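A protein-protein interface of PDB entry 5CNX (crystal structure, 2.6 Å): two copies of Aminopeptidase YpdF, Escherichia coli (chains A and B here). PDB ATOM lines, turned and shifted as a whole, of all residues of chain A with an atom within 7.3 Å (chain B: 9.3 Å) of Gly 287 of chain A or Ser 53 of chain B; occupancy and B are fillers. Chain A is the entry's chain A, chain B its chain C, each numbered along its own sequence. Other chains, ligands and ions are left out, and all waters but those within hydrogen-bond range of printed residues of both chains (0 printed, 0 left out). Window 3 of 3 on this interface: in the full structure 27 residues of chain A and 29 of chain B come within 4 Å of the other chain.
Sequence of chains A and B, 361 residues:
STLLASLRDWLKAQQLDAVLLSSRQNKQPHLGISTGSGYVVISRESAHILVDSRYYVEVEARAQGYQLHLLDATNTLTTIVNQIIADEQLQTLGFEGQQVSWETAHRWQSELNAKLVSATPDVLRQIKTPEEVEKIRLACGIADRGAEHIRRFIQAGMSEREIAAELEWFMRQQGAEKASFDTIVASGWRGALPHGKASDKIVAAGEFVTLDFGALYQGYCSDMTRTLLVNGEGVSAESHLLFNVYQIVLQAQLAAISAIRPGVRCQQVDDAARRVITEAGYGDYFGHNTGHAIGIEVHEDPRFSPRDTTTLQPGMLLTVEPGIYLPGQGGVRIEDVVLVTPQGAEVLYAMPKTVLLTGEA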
ATOM      1  N   ALA A 192     -15.210 -13.364  -9.698  1.00  0.00           N
ATOM      2  CA  ALA A 192     -14.894 -14.783  -9.680  1.00  0.00           C
ATOM      3  C   ALA A 192     -13.944 -15.149 -10.830  1.00  0.00           C
ATOM      4  O   ALA A 192     -13.543 -16.300 -10.968  1.00  0.00           O
ATOM      5  CB  ALA A 192     -16.178 -15.617  -9.750  1.00  0.00           C
ATOM      6  N   LEU A 193     -13.589 -14.164 -11.650  1.00  0.00           N
ATOM      7  CA  LEU A 193     -12.689 -14.387 -12.774  1.00  0.00           C
ATOM      8  C   LEU A 193     -11.306 -13.810 -12.443  1.00  0.00           C
ATOM      9  O   LEU A 193     -11.125 -12.591 -12.486  1.00  0.00           O
ATOM     10  CB  LEU A 193     -13.254 -13.729 -14.034  1.00  0.00           C
ATOM     11  CG  LEU A 193     -14.717 -14.039 -14.383  1.00  0.00           C
ATOM     12  CD1 LEU A 193     -15.201 -13.215 -15.573  1.00  0.00           C
ATOM     13  CD2 LEU A 193     -14.931 -15.512 -14.639  1.00  0.00           C
ATOM     14  N   PRO A 194     -10.322 -14.672 -12.132  1.00  0.00           N
ATOM     15  CA  PRO A 194      -8.999 -14.165 -11.717  1.00  0.00           C
ATOM     16  C   PRO A 194      -8.309 -13.245 -12.735  1.00  0.00           C
ATOM     17  O   PRO A 194      -7.503 -12.387 -12.342  1.00  0.00           O
ATOM     18  CB  PRO A 194      -8.179 -15.450 -11.516  1.00  0.00           C
ATOM     19  CG  PRO A 194      -9.190 -16.499 -11.233  1.00  0.00           C
ATOM     20  CD  PRO A 194     -10.395 -16.142 -12.070  1.00  0.00           C
ATOM     21  N   HIS A 195      -8.657 -13.393 -14.011  1.00  0.00           N
ATOM     22  CA  HIS A 195      -8.078 -12.583 -15.078  1.00  0.00           C
ATOM     23  C   HIS A 195      -9.122 -11.831 -15.849  1.00  0.00           C
ATOM     24  O   HIS A 195      -8.977 -11.605 -17.048  1.00  0.00           O
ATOM     25  CB  HIS A 195      -7.258 -13.440 -16.027  1.00  0.00           C
ATOM     26  CG  HIS A 195      -5.864 -13.666 -15.551  1.00  0.00           C
ATOM     27  ND1 HIS A 195      -4.822 -12.828 -15.901  1.00  0.00           N
ATOM     28  CD2 HIS A 195      -5.342 -14.576 -14.693  1.00  0.00           C
ATOM     29  CE1 HIS A 195      -3.715 -13.241 -15.311  1.00  0.00           C
ATOM     30  NE2 HIS A 195      -4.002 -14.297 -14.566  1.00  0.00           N
ATOM     31  N   ARG A 274      -1.771 -21.131   1.141  1.00  0.00           N
ATOM     32  CA  ARG A 274      -2.724 -22.144   0.720  1.00  0.00           C
ATOM     33  C   ARG A 274      -3.304 -22.887   1.917  1.00  0.00           C
ATOM     34  O   ARG A 274      -4.468 -23.290   1.884  1.00  0.00           O
ATOM     35  CB  ARG A 274      -2.065 -23.127  -0.248  1.00  0.00           C
ATOM     36  CG  ARG A 274      -3.037 -24.000  -1.013  1.00  0.00           C
ATOM     37  CD  ARG A 274      -2.344 -24.736  -2.150  1.00  0.00           C
ATOM     38  NE  ARG A 274      -1.662 -23.797  -3.030  1.00  0.00           N
ATOM     39  CZ  ARG A 274      -2.226 -23.148  -4.044  1.00  0.00           C
ATOM     40  NH1 ARG A 274      -3.508 -23.329  -4.330  1.00  0.00           N
ATOM     41  NH2 ARG A 274      -1.500 -22.307  -4.774  1.00  0.00           N
ATOM     42  N   TYR A 282     -11.787 -23.480   1.608  1.00  0.00           N
ATOM     43  CA  TYR A 282     -11.912 -22.872   0.284  1.00  0.00           C
ATOM     44  C   TYR A 282     -10.793 -23.257  -0.676  1.00  0.00           C
ATOM     45  O   TYR A 282     -10.580 -22.581  -1.687  1.00  0.00           O
ATOM     46  CB  TYR A 282     -11.975 -21.348   0.397  1.00  0.00           C
ATOM     47  CG  TYR A 282     -13.254 -20.820   1.012  1.00  0.00           C
ATOM     48  CD1 TYR A 282     -14.426 -20.720   0.259  1.00  0.00           C
ATOM     49  CD2 TYR A 282     -13.284 -20.387   2.331  1.00  0.00           C
ATOM     50  CE1 TYR A 282     -15.590 -20.221   0.812  1.00  0.00           C
ATOM     51  CE2 TYR A 282     -14.447 -19.890   2.890  1.00  0.00           C
ATOM     52  CZ  TYR A 282     -15.592 -19.806   2.126  1.00  0.00           C
ATOM     53  OH  TYR A 282     -16.735 -19.306   2.691  1.00  0.00           O
ATOM     54  N   GLY A 283     -10.107 -24.359  -0.378  1.00  0.00           N
ATOM     55  CA  GLY A 283      -9.019 -24.833  -1.211  1.00  0.00           C
ATOM     56  C   GLY A 283      -9.399 -25.046  -2.666  1.00  0.00           C
ATOM     57  O   GLY A 283      -8.572 -24.910  -3.568  1.00  0.00           O
ATOM     58  N   ASP A 284     -10.662 -25.350  -2.917  1.00  0.00           N
ATOM     59  CA  ASP A 284     -11.055 -25.674  -4.272  1.00  0.00           C
ATOM     60  C   ASP A 284     -11.307 -24.421  -5.094  1.00  0.00           C
ATOM     61  O   ASP A 284     -11.497 -24.504  -6.306  1.00  0.00           O
ATOM     62  CB  ASP A 284     -12.298 -26.545  -4.256  1.00  0.00           C
ATOM     63  CG  ASP A 284     -12.056 -27.888  -3.595  1.00  0.00           C
ATOM     64  OD1 ASP A 284     -10.921 -28.417  -3.684  1.00  0.00           O
ATOM     65  OD2 ASP A 284     -13.012 -28.416  -2.983  1.00  0.00           O
ATOM     66  N   TYR A 285     -11.280 -23.260  -4.447  1.00  0.00           N
ATOM     67  CA  TYR A 285     -11.493 -22.009  -5.160  1.00  0.00           C
ATOM     68  C   TYR A 285     -10.276 -21.092  -5.128  1.00  0.00           C
ATOM     69  O   TYR A 285     -10.387 -19.878  -5.317  1.00  0.00           O
ATOM     70  CB  TYR A 285     -12.740 -21.306  -4.640  1.00  0.00           C
ATOM     71  CG  TYR A 285     -13.972 -22.139  -4.904  1.00  0.00           C
ATOM     72  CD1 TYR A 285     -14.489 -22.232  -6.192  1.00  0.00           C
ATOM     73  CD2 TYR A 285     -14.621 -22.832  -3.885  1.00  0.00           C
ATOM     74  CE1 TYR A 285     -15.607 -22.993  -6.468  1.00  0.00           C
ATOM     75  CE2 TYR A 285     -15.744 -23.594  -4.150  1.00  0.00           C
ATOM     76  CZ  TYR A 285     -16.235 -23.668  -5.449  1.00  0.00           C
ATOM     77  OH  TYR A 285     -17.362 -24.418  -5.749  1.00  0.00           O
ATOM     78  N   PHE A 286      -9.116 -21.700  -4.886  1.00  0.00           N
ATOM     79  CA  PHE A 286      -7.831 -21.027  -4.953  1.00  0.00           C
ATOM     80  C   PHE A 286      -6.978 -21.828  -5.916  1.00  0.00           C
ATOM     81  O   PHE A 286      -6.151 -22.643  -5.499  1.00  0.00           O
ATOM     82  CB  PHE A 286      -7.162 -20.941  -3.579  1.00  0.00           C
ATOM     83  CG  PHE A 286      -5.795 -20.286  -3.592  1.00  0.00           C
ATOM     84  CD1 PHE A 286      -5.428 -19.400  -4.595  1.00  0.00           C
ATOM     85  CD2 PHE A 286      -4.877 -20.574  -2.604  1.00  0.00           C
ATOM     86  CE1 PHE A 286      -4.171 -18.805  -4.591  1.00  0.00           C
ATOM     87  CE2 PHE A 286      -3.629 -19.981  -2.599  1.00  0.00           C
ATOM     88  CZ  PHE A 286      -3.278 -19.099  -3.591  1.00  0.00           C
ATOM     89  N   GLY A 287      -7.190 -21.610  -7.206  1.00  0.00           N
ATOM     90  CA  GLY A 287      -6.603 -22.476  -8.205  1.00  0.00           C
ATOM     91  C   GLY A 287      -5.246 -22.062  -8.732  1.00  0.00           C
ATOM     92  O   GLY A 287      -4.614 -22.838  -9.446  1.00  0.00           O
ATOM     93  N   HIS A 288      -4.775 -20.866  -8.383  1.00  0.00           N
ATOM     94  CA  HIS A 288      -3.531 -20.399  -8.968  1.00  0.00           C
ATOM     95  C   HIS A 288      -2.388 -20.266  -7.937  1.00  0.00           C
ATOM     96  O   HIS A 288      -2.604 -20.446  -6.731  1.00  0.00           O
ATOM     97  CB  HIS A 288      -3.762 -19.066  -9.687  1.00  0.00           C
ATOM     98  CG  HIS A 288      -4.199 -17.956  -8.793  1.00  0.00           C
ATOM     99  ND1 HIS A 288      -3.319 -17.265  -7.978  1.00  0.00           N
ATOM    100  CD2 HIS A 288      -5.410 -17.376  -8.608  1.00  0.00           C
ATOM    101  CE1 HIS A 288      -3.975 -16.332  -7.317  1.00  0.00           C
ATOM    102  NE2 HIS A 288      -5.249 -16.376  -7.681  1.00  0.00           N
ATOM    103  N   ASN A 289      -1.186 -19.930  -8.416  1.00  0.00           N
ATOM    104  CA  ASN A 289      -0.018 -19.815  -7.551  1.00  0.00           C
ATOM    105  C   ASN A 289      -0.134 -18.677  -6.556  1.00  0.00           C
ATOM    106  O   ASN A 289      -0.890 -17.743  -6.775  1.00  0.00           O
ATOM    107  CB  ASN A 289       1.246 -19.615  -8.392  1.00  0.00           C
ATOM    108  CG  ASN A 289       1.645 -20.859  -9.142  1.00  0.00           C
ATOM    109  OD1 ASN A 289       1.188 -21.962  -8.816  1.00  0.00           O
ATOM    110  ND2 ASN A 289       2.539 -20.705 -10.125  1.00  0.00           N
ATOM    111  N   GLY A 323      -5.969 -15.779  -3.522  1.00  0.00           N
ATOM    112  CA  GLY A 323      -7.330 -15.343  -3.747  1.00  0.00           C
ATOM    113  C   GLY A 323      -8.333 -16.472  -3.633  1.00  0.00           C
ATOM    114  O   GLY A 323      -7.981 -17.651  -3.686  1.00  0.00           O
ATOM    115  N   ILE A 324      -9.593 -16.103  -3.455  1.00  0.00           N
ATOM    116  CA  ILE A 324     -10.684 -17.068  -3.436  1.00  0.00           C
ATOM    117  C   ILE A 324     -11.746 -16.607  -4.419  1.00  0.00           C
ATOM    118  O   ILE A 324     -12.185 -15.462  -4.377  1.00  0.00           O
ATOM    119  CB  ILE A 324     -11.261 -17.222  -2.025  1.00  0.00           C
ATOM    120  CG1 ILE A 324     -10.205 -17.856  -1.106  1.00  0.00           C
ATOM    121  CG2 ILE A 324     -12.530 -18.052  -2.049  1.00  0.00           C
ATOM    122  CD1 ILE A 324     -10.613 -17.967   0.352  1.00  0.00           C
ATOM    123  N   TYR A 325     -12.145 -17.495  -5.314  1.00  0.00           N
ATOM    124  CA  TYR A 325     -13.039 -17.124  -6.399  1.00  0.00           C
ATOM    125  C   TYR A 325     -14.305 -17.984  -6.371  1.00  0.00           C
ATOM    126  O   TYR A 325     -14.247 -19.210  -6.492  1.00  0.00           O
ATOM    127  CB  TYR A 325     -12.291 -17.229  -7.731  1.00  0.00           C
ATOM    128  CG  TYR A 325     -10.951 -16.519  -7.674  1.00  0.00           C
ATOM    129  CD1 TYR A 325     -10.878 -15.141  -7.803  1.00  0.00           C
ATOM    130  CD2 TYR A 325      -9.770 -17.220  -7.458  1.00  0.00           C
ATOM    131  CE1 TYR A 325      -9.677 -14.480  -7.738  1.00  0.00           C
ATOM    132  CE2 TYR A 325      -8.551 -16.567  -7.391  1.00  0.00           C
ATOM    133  CZ  TYR A 325      -8.511 -15.192  -7.530  1.00  0.00           C
ATOM    134  OH  TYR A 325      -7.308 -14.510  -7.459  1.00  0.00           O
ATOM    135  N   SER B  37      -1.402 -18.230 -22.534  1.00  0.00           N
ATOM    136  CA  SER B  37      -1.713 -19.526 -21.941  1.00  0.00           C
ATOM    137  C   SER B  37      -2.806 -20.274 -22.701  1.00  0.00           C
ATOM    138  O   SER B  37      -3.540 -19.688 -23.498  1.00  0.00           O
ATOM    139  CB  SER B  37      -2.155 -19.345 -20.488  1.00  0.00           C
ATOM    140  OG  SER B  37      -1.141 -19.727 -19.588  1.00  0.00           O
ATOM    141  N   LEU B  50      -8.350 -25.845 -23.853  1.00  0.00           N
ATOM    142  CA  LEU B  50      -7.606 -26.212 -22.657  1.00  0.00           C
ATOM    143  C   LEU B  50      -7.177 -24.981 -21.865  1.00  0.00           C
ATOM    144  O   LEU B  50      -6.341 -24.205 -22.341  1.00  0.00           O
ATOM    145  CB  LEU B  50      -6.367 -27.030 -23.020  1.00  0.00           C
ATOM    146  CG  LEU B  50      -6.493 -28.445 -23.586  1.00  0.00           C
ATOM    147  CD1 LEU B  50      -7.038 -28.454 -25.016  1.00  0.00           C
ATOM    148  CD2 LEU B  50      -5.132 -29.136 -23.499  1.00  0.00           C
ATOM    149  N   VAL B  51      -7.740 -24.776 -20.674  1.00  0.00           N
ATOM    150  CA  VAL B  51      -7.292 -23.644 -19.851  1.00  0.00           C
ATOM    151  C   VAL B  51      -7.059 -23.999 -18.379  1.00  0.00           C
ATOM    152  O   VAL B  51      -7.633 -24.960 -17.864  1.00  0.00           O
ATOM    153  CB  VAL B  51      -8.299 -22.455 -19.916  1.00  0.00           C
ATOM    154  CG1 VAL B  51      -8.357 -21.854 -21.301  1.00  0.00           C
ATOM    155  CG2 VAL B  51      -9.665 -22.897 -19.442  1.00  0.00           C
ATOM    156  N   ASP B  52      -6.216 -23.211 -17.706  1.00  0.00           N
ATOM    157  CA  ASP B  52      -6.003 -23.417 -16.277  1.00  0.00           C
ATOM    158  C   ASP B  52      -7.026 -22.600 -15.485  1.00  0.00           C
ATOM    159  O   ASP B  52      -7.779 -21.814 -16.067  1.00  0.00           O
ATOM    160  CB  ASP B  52      -4.558 -23.068 -15.857  1.00  0.00           C
ATOM    161  CG  ASP B  52      -4.159 -21.625 -16.175  1.00  0.00           C
ATOM    162  OD1 ASP B  52      -4.825 -20.675 -15.712  1.00  0.00           O
ATOM    163  OD2 ASP B  52      -3.147 -21.433 -16.877  1.00  0.00           O
ATOM    164  N   SER B  53      -7.014 -22.760 -14.162  1.00  0.00           N
ATOM    165  CA  SER B  53      -8.041 -22.200 -13.278  1.00  0.00           C
ATOM    166  C   SER B  53      -8.217 -20.685 -13.404  1.00  0.00           C
ATOM    167  O   SER B  53      -9.225 -20.134 -12.960  1.00  0.00           O
ATOM    168  CB  SER B  53      -7.719 -22.545 -11.826  1.00  0.00           C
ATOM    169  OG  SER B  53      -6.484 -21.968 -11.430  1.00  0.00           O
ATOM    170  N   ARG B  54      -7.222 -20.011 -13.970  1.00  0.00           N
ATOM    171  CA  ARG B  54      -7.287 -18.565 -14.137  1.00  0.00           C
ATOM    172  C   ARG B  54      -8.304 -18.137 -15.196  1.00  0.00           C
ATOM    173  O   ARG B  54      -8.817 -17.020 -15.131  1.00  0.00           O
ATOM    174  CB  ARG B  54      -5.914 -18.004 -14.475  1.00  0.00           C
ATOM    175  CG  ARG B  54      -4.944 -18.018 -13.303  1.00  0.00           C
ATOM    176  CD  ARG B  54      -3.639 -17.449 -13.761  1.00  0.00           C
ATOM    177  NE  ARG B  54      -3.010 -18.344 -14.719  1.00  0.00           N
ATOM    178  CZ  ARG B  54      -1.914 -18.047 -15.395  1.00  0.00           C
ATOM    179  NH1 ARG B  54      -1.349 -16.859 -15.233  1.00  0.00           N
ATOM    180  NH2 ARG B  54      -1.414 -18.919 -16.254  1.00  0.00           N
ATOM    181  N   TYR B  55      -8.555 -18.992 -16.189  1.00  0.00           N
ATOM    182  CA  TYR B  55      -9.408 -18.607 -17.315  1.00  0.00           C
ATOM    183  C   TYR B  55     -10.649 -19.478 -17.484  1.00  0.00           C
ATOM    184  O   TYR B  55     -11.545 -19.130 -18.256  1.00  0.00           O
ATOM    185  CB  TYR B  55      -8.620 -18.625 -18.635  1.00  0.00           C
ATOM    186  CG  TYR B  55      -7.331 -17.844 -18.620  1.00  0.00           C
ATOM    187  CD1 TYR B  55      -7.345 -16.463 -18.750  1.00  0.00           C
ATOM    188  CD2 TYR B  55      -6.100 -18.482 -18.486  1.00  0.00           C
ATOM    189  CE1 TYR B  55      -6.182 -15.734 -18.740  1.00  0.00           C
ATOM    190  CE2 TYR B  55      -4.920 -17.761 -18.471  1.00  0.00           C
ATOM    191  CZ  TYR B  55      -4.969 -16.383 -18.601  1.00  0.00           C
ATOM    192  OH  TYR B  55      -3.813 -15.630 -18.593  1.00  0.00           O
ATOM    193  N   TYR B  56     -10.723 -20.570 -16.730  1.00  0.00           N
ATOM    194  CA  TYR B  56     -11.751 -21.583 -16.962  1.00  0.00           C
ATOM    195  C   TYR B  56     -13.190 -21.042 -16.932  1.00  0.00           C
ATOM    196  O   TYR B  56     -13.929 -21.188 -17.906  1.00  0.00           O
ATOM    197  CB  TYR B  56     -11.589 -22.699 -15.936  1.00  0.00           C
ATOM    198  CG  TYR B  56     -12.383 -23.946 -16.234  1.00  0.00           C
ATOM    199  CD1 TYR B  56     -11.873 -24.930 -17.067  1.00  0.00           C
ATOM    200  CD2 TYR B  56     -13.631 -24.153 -15.666  1.00  0.00           C
ATOM    201  CE1 TYR B  56     -12.591 -26.081 -17.337  1.00  0.00           C
ATOM    202  CE2 TYR B  56     -14.355 -25.301 -15.928  1.00  0.00           C
ATOM    203  CZ  TYR B  56     -13.827 -26.259 -16.759  1.00  0.00           C
ATOM    204  OH  TYR B  56     -14.542 -27.397 -17.025  1.00  0.00           O
ATOM    205  N   VAL B  57     -13.558 -20.392 -15.830  1.00  0.00           N
ATOM    206  CA  VAL B  57     -14.911 -19.880 -15.601  1.00  0.00           C
ATOM    207  C   VAL B  57     -15.261 -18.811 -16.632  1.00  0.00           C
ATOM    208  O   VAL B  57     -16.425 -18.658 -17.016  1.00  0.00           O
ATOM    209  CB  VAL B  57     -15.071 -19.338 -14.154  1.00  0.00           C
ATOM    210  CG1 VAL B  57     -16.396 -18.657 -13.956  1.00  0.00           C
ATOM    211  CG2 VAL B  57     -14.909 -20.473 -13.154  1.00  0.00           C
ATOM    212  N   GLU B  58     -14.265 -18.042 -17.056  1.00  0.00           N
ATOM    213  CA  GLU B  58     -14.505 -16.984 -18.034  1.00  0.00           C
ATOM    214  C   GLU B  58     -14.681 -17.537 -19.462  1.00  0.00           C
ATOM    215  O   GLU B  58     -15.572 -17.103 -20.211  1.00  0.00           O
ATOM    216  CB  GLU B  58     -13.358 -15.980 -17.992  1.00  0.00           C
ATOM    217  CG  GLU B  58     -13.544 -14.776 -18.873  1.00  0.00           C
ATOM    218  CD  GLU B  58     -12.305 -13.898 -18.938  1.00  0.00           C
ATOM    219  OE1 GLU B  58     -11.262 -14.262 -18.326  1.00  0.00           O
ATOM    220  OE2 GLU B  58     -12.375 -12.841 -19.609  1.00  0.00           O
ATOM    221  N   VAL B  59     -13.865 -18.528 -19.812  1.00  0.00           N
ATOM    222  CA  VAL B  59     -13.910 -19.132 -21.140  1.00  0.00           C
ATOM    223  C   VAL B  59     -15.174 -19.960 -21.277  1.00  0.00           C
ATOM    224  O   VAL B  59     -15.835 -19.916 -22.311  1.00  0.00           O
ATOM    225  CB  VAL B  59     -12.660 -20.011 -21.412  1.00  0.00           C
ATOM    226  CG1 VAL B  59     -12.816 -20.814 -22.691  1.00  0.00           C
ATOM    227  CG2 VAL B  59     -11.420 -19.149 -21.482  1.00  0.00           C
ATOM    228  N   HIS B  69     -11.436 -28.511 -21.174  1.00  0.00           N
ATOM    229  CA  HIS B  69     -10.491 -29.238 -20.325  1.00  0.00           C
ATOM    230  C   HIS B  69      -9.772 -28.297 -19.369  1.00  0.00           C
ATOM    231  O   HIS B  69      -9.294 -27.231 -19.777  1.00  0.00           O
ATOM    232  CB  HIS B  69      -9.447 -29.980 -21.169  1.00  0.00           C
ATOM    233  CG  HIS B  69     -10.032 -30.797 -22.278  1.00  0.00           C
ATOM    234  ND1 HIS B  69     -10.139 -32.165 -22.213  1.00  0.00           N
ATOM    235  CD2 HIS B  69     -10.538 -30.433 -23.481  1.00  0.00           C
ATOM    236  CE1 HIS B  69     -10.690 -32.617 -23.328  1.00  0.00           C
ATOM    237  NE2 HIS B  69     -10.941 -31.585 -24.111  1.00  0.00           N
ATOM    238  N   LEU B  70      -9.702 -28.686 -18.101  1.00  0.00           N
ATOM    239  CA  LEU B  70      -8.952 -27.911 -17.125  1.00  0.00           C
ATOM    240  C   LEU B  70      -7.477 -28.322 -17.110  1.00  0.00           C
ATOM    241  O   LEU B  70      -7.146 -29.506 -17.069  1.00  0.00           O
ATOM    242  CB  LEU B  70      -9.549 -28.061 -15.722  1.00  0.00           C
ATOM    243  CG  LEU B  70      -8.765 -27.330 -14.624  1.00  0.00           C
ATOM    244  CD1 LEU B  70      -8.843 -25.801 -14.804  1.00  0.00           C
ATOM    245  CD2 LEU B  70      -9.210 -27.755 -13.228  1.00  0.00           C
ATOM    246  N   LEU B  71      -6.593 -27.338 -17.153  1.00  0.00           N
ATOM    247  CA  LEU B  71      -5.178 -27.615 -17.007  1.00  0.00           C
ATOM    248  C   LEU B  71      -4.789 -27.530 -15.535  1.00  0.00           C
ATOM    249  O   LEU B  71      -4.982 -26.485 -14.896  1.00  0.00           O
ATOM    250  CB  LEU B  71      -4.329 -26.639 -17.832  1.00  0.00           C
ATOM    251  CG  LEU B  71      -4.331 -26.754 -19.358  1.00  0.00           C
ATOM    252  CD1 LEU B  71      -3.601 -25.566 -19.969  1.00  0.00           C
ATOM    253  CD2 LEU B  71      -3.699 -28.068 -19.809  1.00  0.00           C
ATOM    254  N   ASP B  72      -4.249 -28.621 -14.999  1.00  0.00           N
ATOM    255  CA  ASP B  72      -3.703 -28.601 -13.644  1.00  0.00           C
ATOM    256  C   ASP B  72      -2.457 -29.467 -13.561  1.00  0.00           C
ATOM    257  O   ASP B  72      -1.862 -29.813 -14.583  1.00  0.00           O
ATOM    258  CB  ASP B  72      -4.742 -29.054 -12.609  1.00  0.00           C
ATOM    259  CG  ASP B  72      -5.294 -30.445 -12.883  1.00  0.00           C
ATOM    260  OD1 ASP B  72      -4.545 -31.343 -13.321  1.00  0.00           O
ATOM    261  OD2 ASP B  72      -6.499 -30.647 -12.639  1.00  0.00           O
ATOM    262  N   ALA B  73      -2.055 -29.797 -12.341  1.00  0.00           N
ATOM    263  CA  ALA B  73      -0.876 -30.621 -12.126  1.00  0.00           C
ATOM    264  C   ALA B  73      -1.012 -31.987 -12.790  1.00  0.00           C
ATOM    265  O   ALA B  73      -0.085 -32.470 -13.444  1.00  0.00           O
ATOM    266  CB  ALA B  73      -0.623 -30.782 -10.648  1.00  0.00           C
ATOM    267  N   ASN B  75      -3.629 -32.934 -14.964  1.00  0.00           N
ATOM    268  CA  ASN B  75      -4.128 -32.825 -16.326  1.00  0.00           C
ATOM    269  C   ASN B  75      -3.386 -31.772 -17.138  1.00  0.00           C
ATOM    270  O   ASN B  75      -3.605 -30.571 -16.975  1.00  0.00           O
ATOM    271  CB  ASN B  75      -5.619 -32.516 -16.299  1.00  0.00           C
ATOM    272  CG  ASN B  75      -6.434 -33.675 -15.772  1.00  0.00           C
ATOM    273  OD1 ASN B  75      -7.304 -33.507 -14.917  1.00  0.00           O
ATOM    274  ND2 ASN B  75      -6.144 -34.870 -16.270  1.00  0.00           N
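O of His 288 of chain A is in hydrogen-bond range of NH2 of Arg 274 of chain A (2.9 Å). The side-chain hydroxyl (OH) of Tyr 325 of chain A sits at hydrogen-bond distance from a ring nitrogen (NE2) of His 288 of chain A (2.8 Å). The guanidinium group (NH2) of Arg 54 of chain B is in hydrogen-bond range of the side-chain hydroxyl (OG) of Ser 37 of chain B, at 3.4 Å. The side-chain carboxylate (OD2) of Asp 52 of chain B lies within salt-bridge range of the guanidinium group (NH2) of Arg 54 of chain B, 3.1 Å away.
Of the 17 printed residues of chain B, 5 touch a printed residue of chain A. Hydrophobic or aromatic side chains of chain B that line the printed part of chain A: Tyr 55 and Val 57. Of the 16 printed residues of chain A, 5 touch a printed residue of chain B. Printed residues of chain A that touch a printed residue of chain B: Leu 193, Pro 194, His 195, Gly 287 and His 288. Hydrophobic or aromatic side chains of chain A within 4 Å of the printed part of chain B: Leu 193, Pro 194, His 195 and His 288. Along chain A the printed residues that touch a printed residue of chain B span positions 193 to 288. Among the printed residues, no Asp or Glu carboxylate lies within 4 Å of a Lys or Arg side-chain nitrogen of the other chain.
OG of Ser 53 of chain B sits at hydrogen-bond distance from O of Gly 287 of chain A, 2.9 Å away.
Among the printed residues, pairs that only touch across the chains: His 195 of chain A with Arg 54 of chain B (3.3 Å), Leu 193 of chain A with Val 57 of chain B (3.5 Å), Pro 194 of chain A with Arg 54 of chain B (3.6 Å), Leu 193 of chain A with Glu 58 of chain B (3.6 Å), His 288 of chain A with Ser 53 of chain B (3.7 Å), His 195 of chain A with Tyr 55 of chain B (3.7 Å), His 195 of chain A with Glu 58 of chain B (3.7 Å) and His 288 of chain A with Arg 54 of chain B (3.9 Å).
No position is printed for both chains. Of the 9 pairs that touch across the chains among the printed residues, none has its exchanged pair printed and touching as well.
Ala 192 of chain A touches none of the printed residues of chain B. Of the printed residues of chain B, Leu 193 of chain A touches Val 57 (3.5 Å) and Glu 58 (3.6 Å). Gly 287 of chain A touches just one residue of chain B: Ser 53 (2.9 Å). Printed residues of chain B within 4 Å of His 288 of chain A: Ser 53 and Arg 54. Printed residues of chain A within 4 Å of Ser 53 of chain B: Gly 287 (2.9 Å) and His 288 (3.7 Å). Of the printed residues of chain A, Val 57 of chain B touches Leu 193 (3.5 Å). Of the printed residues of chain A, Glu 58 of chain B touches Leu 193 and His 195. The nearest residue of chain B that does not touch Gly 287 of chain A is Arg 54 of chain B (5.9 Å). The nearest residue of chain A that does not touch Ser 53 of chain B is Pro 194 of chain A (4.02 Å). The nearest printed residue of chain A that does not touch Tyr 55 of chain B is Pro 194 of chain A (5.3 Å).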
